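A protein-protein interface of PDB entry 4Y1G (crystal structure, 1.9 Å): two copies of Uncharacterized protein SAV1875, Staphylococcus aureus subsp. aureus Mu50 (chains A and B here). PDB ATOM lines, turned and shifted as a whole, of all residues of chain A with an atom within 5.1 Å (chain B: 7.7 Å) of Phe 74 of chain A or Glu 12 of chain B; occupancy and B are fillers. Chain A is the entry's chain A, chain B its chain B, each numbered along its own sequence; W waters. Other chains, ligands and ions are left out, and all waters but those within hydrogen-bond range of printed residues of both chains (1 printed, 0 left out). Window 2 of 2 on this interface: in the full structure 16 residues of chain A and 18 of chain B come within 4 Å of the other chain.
A ring nitrogen (NE2) of His 106 of chain A lies within hydrogen-bond range of the side-chain carboxylate (OD2) of Asp 77 of chain B. The side-chain carboxylate of Asp 77 of chain A is in hydrogen-bond range of a ring nitrogen (NE2) of His 106 of chain B (2.9 Å). The backbone carbonyl oxygen (O) of Asp 77 of chain A lies close to the side-chain amide oxygen (OD1) of Asn 127 of chain B, at 2.8 Å.
The backbone carbonyl oxygen of Glu 12 of chain A is in hydrogen-bond range of the backbone NH of Phe 74 of chain A, 2.9 Å away. A ring nitrogen (ND1) of His 106 of chain B is in hydrogen-bond range of OD of CSO 105 of chain B, at 2.8 Å. The backbone NH (N) of Phe 74 of chain B is in hydrogen-bond range of the backbone carbonyl oxygen (O) of Glu 12 of chain B, 2.9 Å away. The backbone NH of Glu 12 of chain B lies within hydrogen-bond range of the backbone carbonyl oxygen of Val 44 of chain B (2.8 Å). O of Glu 12 of chain B is in hydrogen-bond range of N of Ser 75 of chain B (3.5 Å). A ring nitrogen (NE2) of His 78 of chain A is in hydrogen-bond range of the side-chain carboxylate (OE1) of Glu 12 of chain A, at 2.7 Å.
Among the printed residues, pairs that only touch across the chains: Glu 12 of chain A with Phe 74 of chain B (3.5 Å), Phe 74 of chain A with Phe 74 of chain B (3.6 Å), Phe 74 of chain A with Glu 12 of chain B (3.7 Å), Phe 74 of chain A with Asp 77 of chain B (3.7 Å), Phe 74 of chain A with His 78 of chain B (3.7 Å) and Asp 77 of chain A with Phe 74 of chain B (3.8 Å).
Phe 74 of chain A touches just these residues of chain B: Glu 12, Phe 74, Asp 77 and His 78. Glu 12 of chain B touches just one residue of chain A: Phe 74 (3.7 Å). Gly 73 of chain A touches none of the printed residues of chain B. Of the printed residues of chain A, His 106 of chain B touches Asp 77. Printed residues of chain B within 4 Å of Glu 12 of chain A: Phe 74. Of the printed residues of chain A, Phe 74 of chain B touches Glu 12 (3.5 Å), Phe 74 (3.6 Å) and Asp 77 (3.8 Å). Printed residues of chain B within 4 Å of Asp 77 of chain A: Phe 74, His 106 and Asn 127. Asn 11 of chain B touches none of the printed residues of chain A. Leu 9 of chain B touches none of the printed residues of chain A.
Of the 24 printed residues of chain B, 6 touch a printed residue of chain A. Printed residues of chain B that touch a printed residue of chain A: Glu 12, Phe 74, Asp 77, His 78, His 106 and Asn 127. Of the 13 printed residues of chain A, 4 touch a printed residue of chain B. Among the printed residues, 9 pairs touch across the chains. Among the printed residues, no Asp or Glu carboxylate lies within 4 Å of a Lys or Arg side-chain nitrogen of the other chain.
Glu 12 of chain A touches Phe 74 of chain B, and with the chains exchanged Phe 74 of chain A touches Glu 12 of chain B. Phe 74 of chain A touches its own counterpart, Phe 74 of chain B. Phe 74 of chain A touches Asp 77 of chain B, and with the chains exchanged Asp 77 of chain A touches Phe 74 of chain B. Phe 74 of chain A touches His 78 of chain B, but with the chains exchanged His 78 of chain A does not touch Phe 74 of chain B (4.04 Å). Positions printed for both chains: 11, 12, 13, 14, 46, 72, 73, 74, 75, 76, 77, 78 and 106.
Water W1 lies within hydrogen-bond range of the side-chain carboxylate of Asp 77 of chain A (2.7 Å) and the backbone carbonyl oxygen of Asn 127 of chain B (2.9 Å).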
ATOM      1  N   ASN A  11      -3.591  -3.565   6.441  1.00  0.00           N
ATOM      2  CA  ASN A  11      -2.413  -4.178   7.041  1.00  0.00           C
ATOM      3  C   ASN A  11      -2.725  -5.105   8.209  1.00  0.00           C
ATOM      4  O   ASN A  11      -3.678  -4.867   8.954  1.00  0.00           O
ATOM      5  CB  ASN A  11      -1.432  -3.088   7.495  1.00  0.00           C
ATOM      6  CG  ASN A  11      -0.737  -2.421   6.324  1.00  0.00           C
ATOM      7  OD1 ASN A  11      -0.191  -3.102   5.450  1.00  0.00           O
ATOM      8  ND2 ASN A  11      -0.988  -1.126   6.167  1.00  0.00           N
ATOM      9  N   GLU A  12      -1.818  -6.057   8.440  1.00  0.00           N
ATOM     10  CA  GLU A  12      -1.812  -6.932   9.628  1.00  0.00           C
ATOM     11  C   GLU A  12      -2.978  -7.910   9.624  1.00  0.00           C
ATOM     12  O   GLU A  12      -3.340  -8.462  10.659  1.00  0.00           O
ATOM     13  CB  GLU A  12      -1.796  -6.119  10.923  1.00  0.00           C
ATOM     14  CG  GLU A  12      -0.579  -5.217  11.050  1.00  0.00           C
ATOM     15  CD  GLU A  12      -0.480  -4.580  12.418  1.00  0.00           C
ATOM     16  OE1 GLU A  12      -1.287  -3.675  12.715  1.00  0.00           O
ATOM     17  OE2 GLU A  12       0.433  -4.952  13.180  1.00  0.00           O
ATOM     18  N   PHE A  13      -3.437  -8.266   8.436  1.00  0.00           N
ATOM     19  CA  PHE A  13      -4.310  -9.421   8.310  1.00  0.00           C
ATOM     20  C   PHE A  13      -3.527 -10.692   8.665  1.00  0.00           C
ATOM     21  O   PHE A  13      -2.289 -10.750   8.532  1.00  0.00           O
ATOM     22  CB  PHE A  13      -4.860  -9.520   6.883  1.00  0.00           C
ATOM     23  CG  PHE A  13      -3.800  -9.674   5.839  1.00  0.00           C
ATOM     24  CD1 PHE A  13      -3.176  -8.560   5.305  1.00  0.00           C
ATOM     25  CD2 PHE A  13      -3.543 -10.910   5.278  1.00  0.00           C
ATOM     26  CE1 PHE A  13      -2.220  -8.689   4.314  1.00  0.00           C
ATOM     27  CE2 PHE A  13      -2.585 -11.047   4.295  1.00  0.00           C
ATOM     28  CZ  PHE A  13      -1.950  -9.933   3.788  1.00  0.00           C
ATOM     29  N   GLU A  14      -4.244 -11.706   9.130  1.00  0.00           N
ATOM     30  CA  GLU A  14      -3.630 -13.006   9.364  1.00  0.00           C
ATOM     31  C   GLU A  14      -3.393 -13.693   8.015  1.00  0.00           C
ATOM     32  O   GLU A  14      -4.341 -13.961   7.272  1.00  0.00           O
ATOM     33  CB  GLU A  14      -4.514 -13.856  10.278  1.00  0.00           C
ATOM     34  CG  GLU A  14      -3.946 -15.232  10.625  1.00  0.00           C
ATOM     35  CD  GLU A  14      -2.795 -15.145  11.621  1.00  0.00           C
ATOM     36  OE1 GLU A  14      -3.031 -14.740  12.774  1.00  0.00           O
ATOM     37  OE2 GLU A  14      -1.635 -15.369  11.226  1.00  0.00           O
ATOM     38  N   LYS A  46       0.394  -9.976   9.010  1.00  0.00           N
ATOM     39  CA  LYS A  46       1.139 -10.043  10.273  1.00  0.00           C
ATOM     40  C   LYS A  46       2.454 -10.781  10.095  1.00  0.00           C
ATOM     41  O   LYS A  46       3.407 -10.552  10.833  1.00  0.00           O
ATOM     42  CB  LYS A  46       0.329 -10.770  11.340  1.00  0.00           C
ATOM     43  CG  LYS A  46      -0.984 -10.120  11.684  1.00  0.00           C
ATOM     44  CD  LYS A  46      -1.706 -10.992  12.685  1.00  0.00           C
ATOM     45  CE  LYS A  46      -0.722 -11.549  13.692  1.00  0.00           C
ATOM     46  NZ  LYS A  46      -1.447 -11.956  14.922  1.00  0.00           N
ATOM     47  N   GLY A  72      -9.282 -12.219   8.864  1.00  0.00           N
ATOM     48  CA  GLY A  72      -9.055 -11.682  10.191  1.00  0.00           C
ATOM     49  C   GLY A  72      -7.645 -11.152  10.454  1.00  0.00           C
ATOM     50  O   GLY A  72      -7.130 -10.321   9.707  1.00  0.00           O
ATOM     51  N   GLY A  73      -7.113 -11.473  11.630  1.00  0.00           N
ATOM     52  CA  GLY A  73      -5.974 -10.723  12.158  1.00  0.00           C
ATOM     53  C   GLY A  73      -6.405  -9.377  12.705  1.00  0.00           C
ATOM     54  O   GLY A  73      -7.525  -9.229  13.235  1.00  0.00           O
ATOM     55  N   PHE A  74      -5.540  -8.381  12.558  1.00  0.00           N
ATOM     56  CA  PHE A  74      -5.887  -7.035  12.985  1.00  0.00           C
ATOM     57  C   PHE A  74      -6.334  -6.153  11.809  1.00  0.00           C
ATOM     58  O   PHE A  74      -6.599  -4.952  11.964  1.00  0.00           O
ATOM     59  CB  PHE A  74      -4.713  -6.405  13.744  1.00  0.00           C
ATOM     60  CG  PHE A  74      -4.385  -7.118  15.035  1.00  0.00           C
ATOM     61  CD1 PHE A  74      -5.379  -7.398  15.953  1.00  0.00           C
ATOM     62  CD2 PHE A  74      -3.097  -7.570  15.293  1.00  0.00           C
ATOM     63  CE1 PHE A  74      -5.107  -8.119  17.104  1.00  0.00           C
ATOM     64  CE2 PHE A  74      -2.807  -8.249  16.474  1.00  0.00           C
ATOM     65  CZ  PHE A  74      -3.823  -8.564  17.349  1.00  0.00           C
ATOM     66  N   SER A  75      -6.491  -6.759  10.647  1.00  0.00           N
ATOM     67  CA  SER A  75      -6.999  -6.010   9.501  1.00  0.00           C
ATOM     68  C   SER A  75      -8.422  -5.440   9.748  1.00  0.00           C
ATOM     69  O   SER A  75      -8.642  -4.234   9.561  1.00  0.00           O
ATOM     70  CB  SER A  75      -6.934  -6.885   8.242  1.00  0.00           C
ATOM     71  OG  SER A  75      -7.803  -6.419   7.236  1.00  0.00           O
ATOM     72  N   PRO A  76      -9.349  -6.254  10.303  1.00  0.00           N
ATOM     73  CA  PRO A  76     -10.672  -5.678  10.578  1.00  0.00           C
ATOM     74  C   PRO A  76     -10.655  -4.505  11.551  1.00  0.00           C
ATOM     75  O   PRO A  76     -11.270  -3.482  11.265  1.00  0.00           O
ATOM     76  CB  PRO A  76     -11.456  -6.855  11.176  1.00  0.00           C
ATOM     77  CG  PRO A  76     -10.835  -8.053  10.533  1.00  0.00           C
ATOM     78  CD  PRO A  76      -9.351  -7.716  10.506  1.00  0.00           C
ATOM     79  N   ASP A  77      -9.771  -4.541  12.547  1.00  0.00           N
ATOM     80  CA  ASP A  77      -9.637  -3.381  13.435  1.00  0.00           C
ATOM     81  C   ASP A  77      -9.180  -2.118  12.694  1.00  0.00           C
ATOM     82  O   ASP A  77      -9.742  -1.025  12.872  1.00  0.00           O
ATOM     83  CB  ASP A  77      -8.694  -3.679  14.593  1.00  0.00           C
ATOM     84  CG  ASP A  77      -8.738  -2.597  15.663  1.00  0.00           C
ATOM     85  OD1 ASP A  77      -9.626  -2.650  16.539  1.00  0.00           O
ATOM     86  OD2 ASP A  77      -7.940  -1.648  15.576  1.00  0.00           O
ATOM     87  N   HIS A  78      -8.190  -2.265  11.823  1.00  0.00           N
ATOM     88  CA  HIS A  78      -7.762  -1.120  11.006  1.00  0.00           C
ATOM     89  C   HIS A  78      -8.865  -0.580  10.140  1.00  0.00           C
ATOM     90  O   HIS A  78      -8.959   0.634   9.921  1.00  0.00           O
ATOM     91  CB  HIS A  78      -6.554  -1.478  10.149  1.00  0.00           C
ATOM     92  CG  HIS A  78      -5.282  -1.624  10.933  1.00  0.00           C
ATOM     93  ND1 HIS A  78      -4.884  -0.707  11.844  1.00  0.00           N
ATOM     94  CD2 HIS A  78      -4.351  -2.658  10.982  1.00  0.00           C
ATOM     95  CE1 HIS A  78      -3.722  -1.107  12.401  1.00  0.00           C
ATOM     96  NE2 HIS A  78      -3.389  -2.295  11.861  1.00  0.00           N
ATOM     97  N   HIS A 106     -11.090 -12.635  13.464  1.00  0.00           N
ATOM     98  CA  HIS A 106     -11.600 -11.286  13.753  1.00  0.00           C
ATOM     99  C   HIS A 106     -12.508 -10.683  12.687  1.00  0.00           C
ATOM    100  O   HIS A 106     -13.096  -9.622  12.901  1.00  0.00           O
ATOM    101  CB  HIS A 106     -10.430 -10.316  13.991  1.00  0.00           C
ATOM    102  CG  HIS A 106      -9.769 -10.487  15.338  1.00  0.00           C
ATOM    103  ND1 HIS A 106      -8.830 -11.434  15.578  1.00  0.00           N
ATOM    104  CD2 HIS A 106      -9.921  -9.774  16.526  1.00  0.00           C
ATOM    105  CE1 HIS A 106      -8.384 -11.303  16.846  1.00  0.00           C
ATOM    106  NE2 HIS A 106      -9.040 -10.279  17.416  1.00  0.00           N
ATOM    107  N   LEU B   9      -1.464  -6.350  30.986  1.00  0.00           N
ATOM    108  CA  LEU B   9      -0.593  -6.146  29.841  1.00  0.00           C
ATOM    109  C   LEU B   9      -0.297  -7.453  29.117  1.00  0.00           C
ATOM    110  O   LEU B   9       0.102  -8.452  29.734  1.00  0.00           O
ATOM    111  CB  LEU B   9       0.712  -5.478  30.293  1.00  0.00           C
ATOM    112  CG  LEU B   9       1.353  -4.573  29.235  1.00  0.00           C
ATOM    113  CD1 LEU B   9       0.444  -3.377  28.961  1.00  0.00           C
ATOM    114  CD2 LEU B   9       2.728  -4.111  29.722  1.00  0.00           C
ATOM    115  N   ALA B  10      -0.498  -7.454  27.807  1.00  0.00           N
ATOM    116  CA  ALA B  10       0.000  -8.524  26.959  1.00  0.00           C
ATOM    117  C   ALA B  10       0.960  -7.953  25.933  1.00  0.00           C
ATOM    118  O   ALA B  10       1.155  -6.733  25.875  1.00  0.00           O
ATOM    119  CB  ALA B  10      -1.161  -9.239  26.268  1.00  0.00           C
ATOM    120  N   ASN B  11       1.433  -8.808  25.023  1.00  0.00           N
ATOM    121  CA  ASN B  11       2.208  -8.338  23.872  1.00  0.00           C
ATOM    122  C   ASN B  11       1.447  -7.326  23.027  1.00  0.00           C
ATOM    123  O   ASN B  11       0.212  -7.376  22.936  1.00  0.00           O
ATOM    124  CB  ASN B  11       2.681  -9.519  23.004  1.00  0.00           C
ATOM    125  CG  ASN B  11       3.821 -10.297  23.651  1.00  0.00           C
ATOM    126  OD1 ASN B  11       4.818  -9.726  24.075  1.00  0.00           O
ATOM    127  ND2 ASN B  11       3.670 -11.609  23.728  1.00  0.00           N
ATOM    128  N   GLU B  12       2.193  -6.436  22.377  1.00  0.00           N
ATOM    129  CA  GLU B  12       1.644  -5.494  21.398  1.00  0.00           C
ATOM    130  C   GLU B  12       0.776  -4.398  22.017  1.00  0.00           C
ATOM    131  O   GLU B  12      -0.023  -3.777  21.323  1.00  0.00           O
ATOM    132  CB  GLU B  12       0.879  -6.221  20.269  1.00  0.00           C
ATOM    133  CG  GLU B  12       1.698  -7.282  19.543  1.00  0.00           C
ATOM    134  CD  GLU B  12       0.969  -7.832  18.322  1.00  0.00           C
ATOM    135  OE1 GLU B  12       0.226  -8.826  18.456  1.00  0.00           O
ATOM    136  OE2 GLU B  12       0.995  -7.164  17.272  1.00  0.00           O
ATOM    137  N   PHE B  13       1.054  -4.060  23.274  1.00  0.00           N
ATOM    138  CA  PHE B  13       0.570  -2.814  23.837  1.00  0.00           C
ATOM    139  C   PHE B  13       1.208  -1.615  23.126  1.00  0.00           C
ATOM    140  O   PHE B  13       2.312  -1.701  22.554  1.00  0.00           O
ATOM    141  CB  PHE B  13       0.848  -2.771  25.347  1.00  0.00           C
ATOM    142  CG  PHE B  13       2.313  -2.806  25.704  1.00  0.00           C
ATOM    143  CD1 PHE B  13       2.995  -4.017  25.829  1.00  0.00           C
ATOM    144  CD2 PHE B  13       3.015  -1.619  25.912  1.00  0.00           C
ATOM    145  CE1 PHE B  13       4.343  -4.039  26.195  1.00  0.00           C
ATOM    146  CE2 PHE B  13       4.348  -1.634  26.276  1.00  0.00           C
ATOM    147  CZ  PHE B  13       5.027  -2.843  26.381  1.00  0.00           C
ATOM    148  N   GLU B  14       0.463  -0.525  23.059  1.00  0.00           N
ATOM    149  CA  GLU B  14       1.012   0.719  22.544  1.00  0.00           C
ATOM    150  C   GLU B  14       1.995   1.286  23.564  1.00  0.00           C
ATOM    151  O   GLU B  14       1.615   1.564  24.712  1.00  0.00           O
ATOM    152  CB  GLU B  14      -0.120   1.724  22.297  1.00  0.00           C
ATOM    153  CG  GLU B  14       0.367   3.031  21.716  1.00  0.00           C
ATOM    154  CD  GLU B  14       0.897   2.858  20.309  1.00  0.00           C
ATOM    155  OE1 GLU B  14       0.192   2.256  19.475  1.00  0.00           O
ATOM    156  OE2 GLU B  14       2.074   3.183  20.087  1.00  0.00           O
ATOM    157  N   ASP B  15       3.273   1.348  23.180  1.00  0.00           N
ATOM    158  CA  ASP B  15       4.351   1.633  24.130  1.00  0.00           C
ATOM    159  C   ASP B  15       4.018   2.838  25.030  1.00  0.00           C
ATOM    160  O   ASP B  15       4.067   2.715  26.261  1.00  0.00           O
ATOM    161  CB  ASP B  15       5.678   1.866  23.393  1.00  0.00           C
ATOM    162  CG  ASP B  15       6.129   0.650  22.584  1.00  0.00           C
ATOM    163  OD1 ASP B  15       5.273  -0.010  21.962  1.00  0.00           O
ATOM    164  OD2 ASP B  15       7.354   0.454  22.444  1.00  0.00           O
ATOM    165  N   VAL B  43       6.790  -8.936  28.161  1.00  0.00           N
ATOM    166  CA  VAL B  43       5.913  -8.591  27.053  1.00  0.00           C
ATOM    167  C   VAL B  43       6.494  -7.417  26.289  1.00  0.00           C
ATOM    168  O   VAL B  43       7.275  -6.639  26.829  1.00  0.00           O
ATOM    169  CB  VAL B  43       4.474  -8.303  27.510  1.00  0.00           C
ATOM    170  CG1 VAL B  43       3.833  -9.586  28.031  1.00  0.00           C
ATOM    171  CG2 VAL B  43       4.467  -7.216  28.573  1.00  0.00           C
ATOM    172  N   VAL B  44       6.258  -7.401  24.985  1.00  0.00           N
ATOM    173  CA  VAL B  44       6.938  -6.460  24.128  1.00  0.00           C
ATOM    174  C   VAL B  44       5.915  -5.604  23.380  1.00  0.00           C
ATOM    175  O   VAL B  44       4.982  -6.139  22.784  1.00  0.00           O
ATOM    176  CB  VAL B  44       7.842  -7.201  23.116  1.00  0.00           C
ATOM    177  CG1 VAL B  44       8.499  -6.195  22.168  1.00  0.00           C
ATOM    178  CG2 VAL B  44       8.898  -8.026  23.867  1.00  0.00           C
ATOM    179  N   GLY B  45       6.109  -4.288  23.409  1.00  0.00           N
ATOM    180  CA  GLY B  45       5.171  -3.336  22.807  1.00  0.00           C
ATOM    181  C   GLY B  45       5.242  -3.295  21.296  1.00  0.00           C
ATOM    182  O   GLY B  45       6.160  -3.836  20.693  1.00  0.00           O
ATOM    183  N   LYS B  46       4.278  -2.625  20.673  1.00  0.00           N
ATOM    184  CA  LYS B  46       4.296  -2.459  19.222  1.00  0.00           C
ATOM    185  C   LYS B  46       5.618  -1.885  18.712  1.00  0.00           C
ATOM    186  O   LYS B  46       6.019  -2.164  17.588  1.00  0.00           O
ATOM    187  CB  LYS B  46       3.156  -1.558  18.777  1.00  0.00           C
ATOM    188  CG  LYS B  46       1.786  -2.068  19.165  1.00  0.00           C
ATOM    189  CD  LYS B  46       0.716  -1.100  18.686  1.00  0.00           C
ATOM    190  CE  LYS B  46       0.345  -1.370  17.241  1.00  0.00           C
ATOM    191  NZ  LYS B  46      -1.137  -1.441  17.105  1.00  0.00           N
ATOM    192  N   HIS B  47       6.244  -1.016  19.499  1.00  0.00           N
ATOM    193  CA  HIS B  47       7.489  -0.364  19.071  1.00  0.00           C
ATOM    194  C   HIS B  47       8.699  -0.863  19.806  1.00  0.00           C
ATOM    195  O   HIS B  47       9.752  -0.226  19.782  1.00  0.00           O
ATOM    196  CB  HIS B  47       7.373   1.153  19.197  1.00  0.00           C
ATOM    197  CG  HIS B  47       6.199   1.731  18.446  1.00  0.00           C
ATOM    198  ND1 HIS B  47       6.128   1.707  17.099  1.00  0.00           N
ATOM    199  CD2 HIS B  47       4.962   2.185  18.895  1.00  0.00           C
ATOM    200  CE1 HIS B  47       4.921   2.158  16.704  1.00  0.00           C
ATOM    201  NE2 HIS B  47       4.213   2.464  17.802  1.00  0.00           N
ATOM    202  N   GLU B  49       9.247  -1.736  23.140  1.00  0.00           N
ATOM    203  CA  GLU B  49       9.460  -1.587  24.577  1.00  0.00           C
ATOM    204  C   GLU B  49       9.262  -2.904  25.319  1.00  0.00           C
ATOM    205  O   GLU B  49       8.281  -3.605  25.095  1.00  0.00           O
ATOM    206  CB  GLU B  49       8.562  -0.516  25.198  1.00  0.00           C
ATOM    207  CG  GLU B  49       8.880  -0.361  26.676  1.00  0.00           C
ATOM    208  CD  GLU B  49       8.163   0.783  27.336  1.00  0.00           C
ATOM    209  OE1 GLU B  49       7.309   1.407  26.674  1.00  0.00           O
ATOM    210  OE2 GLU B  49       8.349   0.951  28.564  1.00  0.00           O
ATOM    211  N   PRO B  71      -3.581  -0.255  29.325  1.00  0.00           N
ATOM    212  CA  PRO B  71      -2.999   0.386  28.157  1.00  0.00           C
ATOM    213  C   PRO B  71      -3.585  -0.198  26.860  1.00  0.00           C
ATOM    214  O   PRO B  71      -4.088  -1.323  26.853  1.00  0.00           O
ATOM    215  CB  PRO B  71      -1.498   0.051  28.282  1.00  0.00           C
ATOM    216  CG  PRO B  71      -1.273  -0.160  29.762  1.00  0.00           C
ATOM    217  CD  PRO B  71      -2.551  -0.840  30.221  1.00  0.00           C
ATOM    218  N   GLY B  72      -3.629   0.601  25.807  1.00  0.00           N
ATOM    219  CA  GLY B  72      -4.184   0.140  24.538  1.00  0.00           C
ATOM    220  C   GLY B  72      -3.172  -0.525  23.608  1.00  0.00           C
ATOM    221  O   GLY B  72      -2.387  -1.392  24.033  1.00  0.00           O
ATOM    222  N   GLY B  73      -3.314  -0.258  22.309  1.00  0.00           N
ATOM    223  CA  GLY B  73      -2.708  -1.117  21.280  1.00  0.00           C
ATOM    224  C   GLY B  73      -3.504  -2.402  21.092  1.00  0.00           C
ATOM    225  O   GLY B  73      -4.732  -2.408  21.217  1.00  0.00           O
ATOM    226  N   PHE B  74      -2.820  -3.489  20.747  1.00  0.00           N
ATOM    227  CA  PHE B  74      -3.501  -4.774  20.584  1.00  0.00           C
ATOM    228  C   PHE B  74      -3.388  -5.647  21.816  1.00  0.00           C
ATOM    229  O   PHE B  74      -3.923  -6.751  21.841  1.00  0.00           O
ATOM    230  CB  PHE B  74      -2.987  -5.520  19.352  1.00  0.00           C
ATOM    231  CG  PHE B  74      -3.303  -4.818  18.059  1.00  0.00           C
ATOM    232  CD1 PHE B  74      -4.550  -4.248  17.862  1.00  0.00           C
ATOM    233  CD2 PHE B  74      -2.314  -4.599  17.116  1.00  0.00           C
ATOM    234  CE1 PHE B  74      -4.821  -3.520  16.709  1.00  0.00           C
ATOM    235  CE2 PHE B  74      -2.601  -3.929  15.933  1.00  0.00           C
ATOM    236  CZ  PHE B  74      -3.831  -3.341  15.763  1.00  0.00           C
ATOM    237  N   SER B  75      -2.841  -5.087  22.884  1.00  0.00           N
ATOM    238  CA  SER B  75      -2.747  -5.819  24.144  1.00  0.00           C
ATOM    239  C   SER B  75      -4.147  -6.220  24.675  1.00  0.00           C
ATOM    240  O   SER B  75      -4.362  -7.382  25.059  1.00  0.00           O
ATOM    241  CB  SER B  75      -1.922  -5.005  25.177  1.00  0.00           C
ATOM    242  OG  SER B  75      -2.088  -5.491  26.508  1.00  0.00           O
ATOM    243  N   PRO B  76      -5.111  -5.278  24.688  1.00  0.00           N
ATOM    244  CA  PRO B  76      -6.414  -5.671  25.211  1.00  0.00           C
ATOM    245  C   PRO B  76      -7.057  -6.774  24.391  1.00  0.00           C
ATOM    246  O   PRO B  76      -7.639  -7.698  24.960  1.00  0.00           O
ATOM    247  CB  PRO B  76      -7.239  -4.385  25.100  1.00  0.00           C
ATOM    248  CG  PRO B  76      -6.215  -3.295  25.241  1.00  0.00           C
ATOM    249  CD  PRO B  76      -5.063  -3.829  24.412  1.00  0.00           C
ATOM    250  N   ASP B  77      -6.905  -6.733  23.070  1.00  0.00           N
ATOM    251  CA  ASP B  77      -7.437  -7.842  22.261  1.00  0.00           C
ATOM    252  C   ASP B  77      -6.807  -9.187  22.665  1.00  0.00           C
ATOM    253  O   ASP B  77      -7.518 -10.177  22.878  1.00  0.00           O
ATOM    254  CB  ASP B  77      -7.264  -7.584  20.767  1.00  0.00           C
ATOM    255  CG  ASP B  77      -7.972  -8.623  19.918  1.00  0.00           C
ATOM    256  OD1 ASP B  77      -9.189  -8.483  19.673  1.00  0.00           O
ATOM    257  OD2 ASP B  77      -7.341  -9.649  19.626  1.00  0.00           O
ATOM    258  N   HIS B  78      -5.487  -9.208  22.838  1.00  0.00           N
ATOM    259  CA  HIS B  78      -4.831 -10.404  23.353  1.00  0.00           C
ATOM    260  C   HIS B  78      -5.401 -10.852  24.672  1.00  0.00           C
ATOM    261  O   HIS B  78      -5.655 -12.049  24.883  1.00  0.00           O
ATOM    262  CB  HIS B  78      -3.321 -10.207  23.445  1.00  0.00           C
ATOM    263  CG  HIS B  78      -2.635 -10.153  22.104  1.00  0.00           C
ATOM    264  ND1 HIS B  78      -2.923 -11.016  21.110  1.00  0.00           N
ATOM    265  CD2 HIS B  78      -1.735  -9.232  21.572  1.00  0.00           C
ATOM    266  CE1 HIS B  78      -2.226 -10.679  20.002  1.00  0.00           C
ATOM    267  NE2 HIS B  78      -1.485  -9.605  20.288  1.00  0.00           N
ATOM    268  N   CSO B 105      -7.357   4.355  24.583  1.00  0.00           N
ATOM    269  CA  CSO B 105      -7.192   3.839  23.187  1.00  0.00           C
ATOM    270  CB  CSO B 105      -5.676   3.653  22.919  1.00  0.00           C
ATOM    271  SG  CSO B 105      -5.118   3.299  21.257  1.00  0.00           S
ATOM    272  C   CSO B 105      -8.094   2.629  22.992  1.00  0.00           C
ATOM    273  O   CSO B 105      -9.313   2.758  23.119  1.00  0.00           O
ATOM    274  OD  CSO B 105      -4.831   1.603  21.398  1.00  0.00           O
ATOM    275  N   HIS B 106      -7.518   1.435  22.792  1.00  0.00           N
ATOM    276  CA  HIS B 106      -8.270   0.157  22.830  1.00  0.00           C
ATOM    277  C   HIS B 106      -8.551  -0.373  24.217  1.00  0.00           C
ATOM    278  O   HIS B 106      -9.322  -1.315  24.378  1.00  0.00           O
ATOM    279  CB  HIS B 106      -7.531  -0.942  22.047  1.00  0.00           C
ATOM    280  CG  HIS B 106      -7.557  -0.752  20.553  1.00  0.00           C
ATOM    281  ND1 HIS B 106      -6.763   0.134  19.921  1.00  0.00           N
ATOM    282  CD2 HIS B 106      -8.280  -1.413  19.557  1.00  0.00           C
ATOM    283  CE1 HIS B 106      -7.007   0.082  18.601  1.00  0.00           C
ATOM    284  NE2 HIS B 106      -7.929  -0.867  18.383  1.00  0.00           N
ATOM    285  N   ASN B 127     -11.961   3.116  16.598  1.00  0.00           N
ATOM    286  CA  ASN B 127     -12.106   1.724  16.134  1.00  0.00           C
ATOM    287  C   ASN B 127     -13.007   0.859  17.052  1.00  0.00           C
ATOM    288  O   ASN B 127     -13.449  -0.222  16.654  1.00  0.00           O
ATOM    289  CB  ASN B 127     -10.722   1.037  16.015  1.00  0.00           C
ATOM    290  CG  ASN B 127      -9.718   1.859  15.216  1.00  0.00           C
ATOM    291  OD1 ASN B 127      -9.090   1.356  14.266  1.00  0.00           O
ATOM    292  ND2 ASN B 127      -9.501   3.091  15.638  1.00  0.00           N
HETATM  293  O   HOH W   1     -12.240  -2.820  16.114  1.00  0.00           O
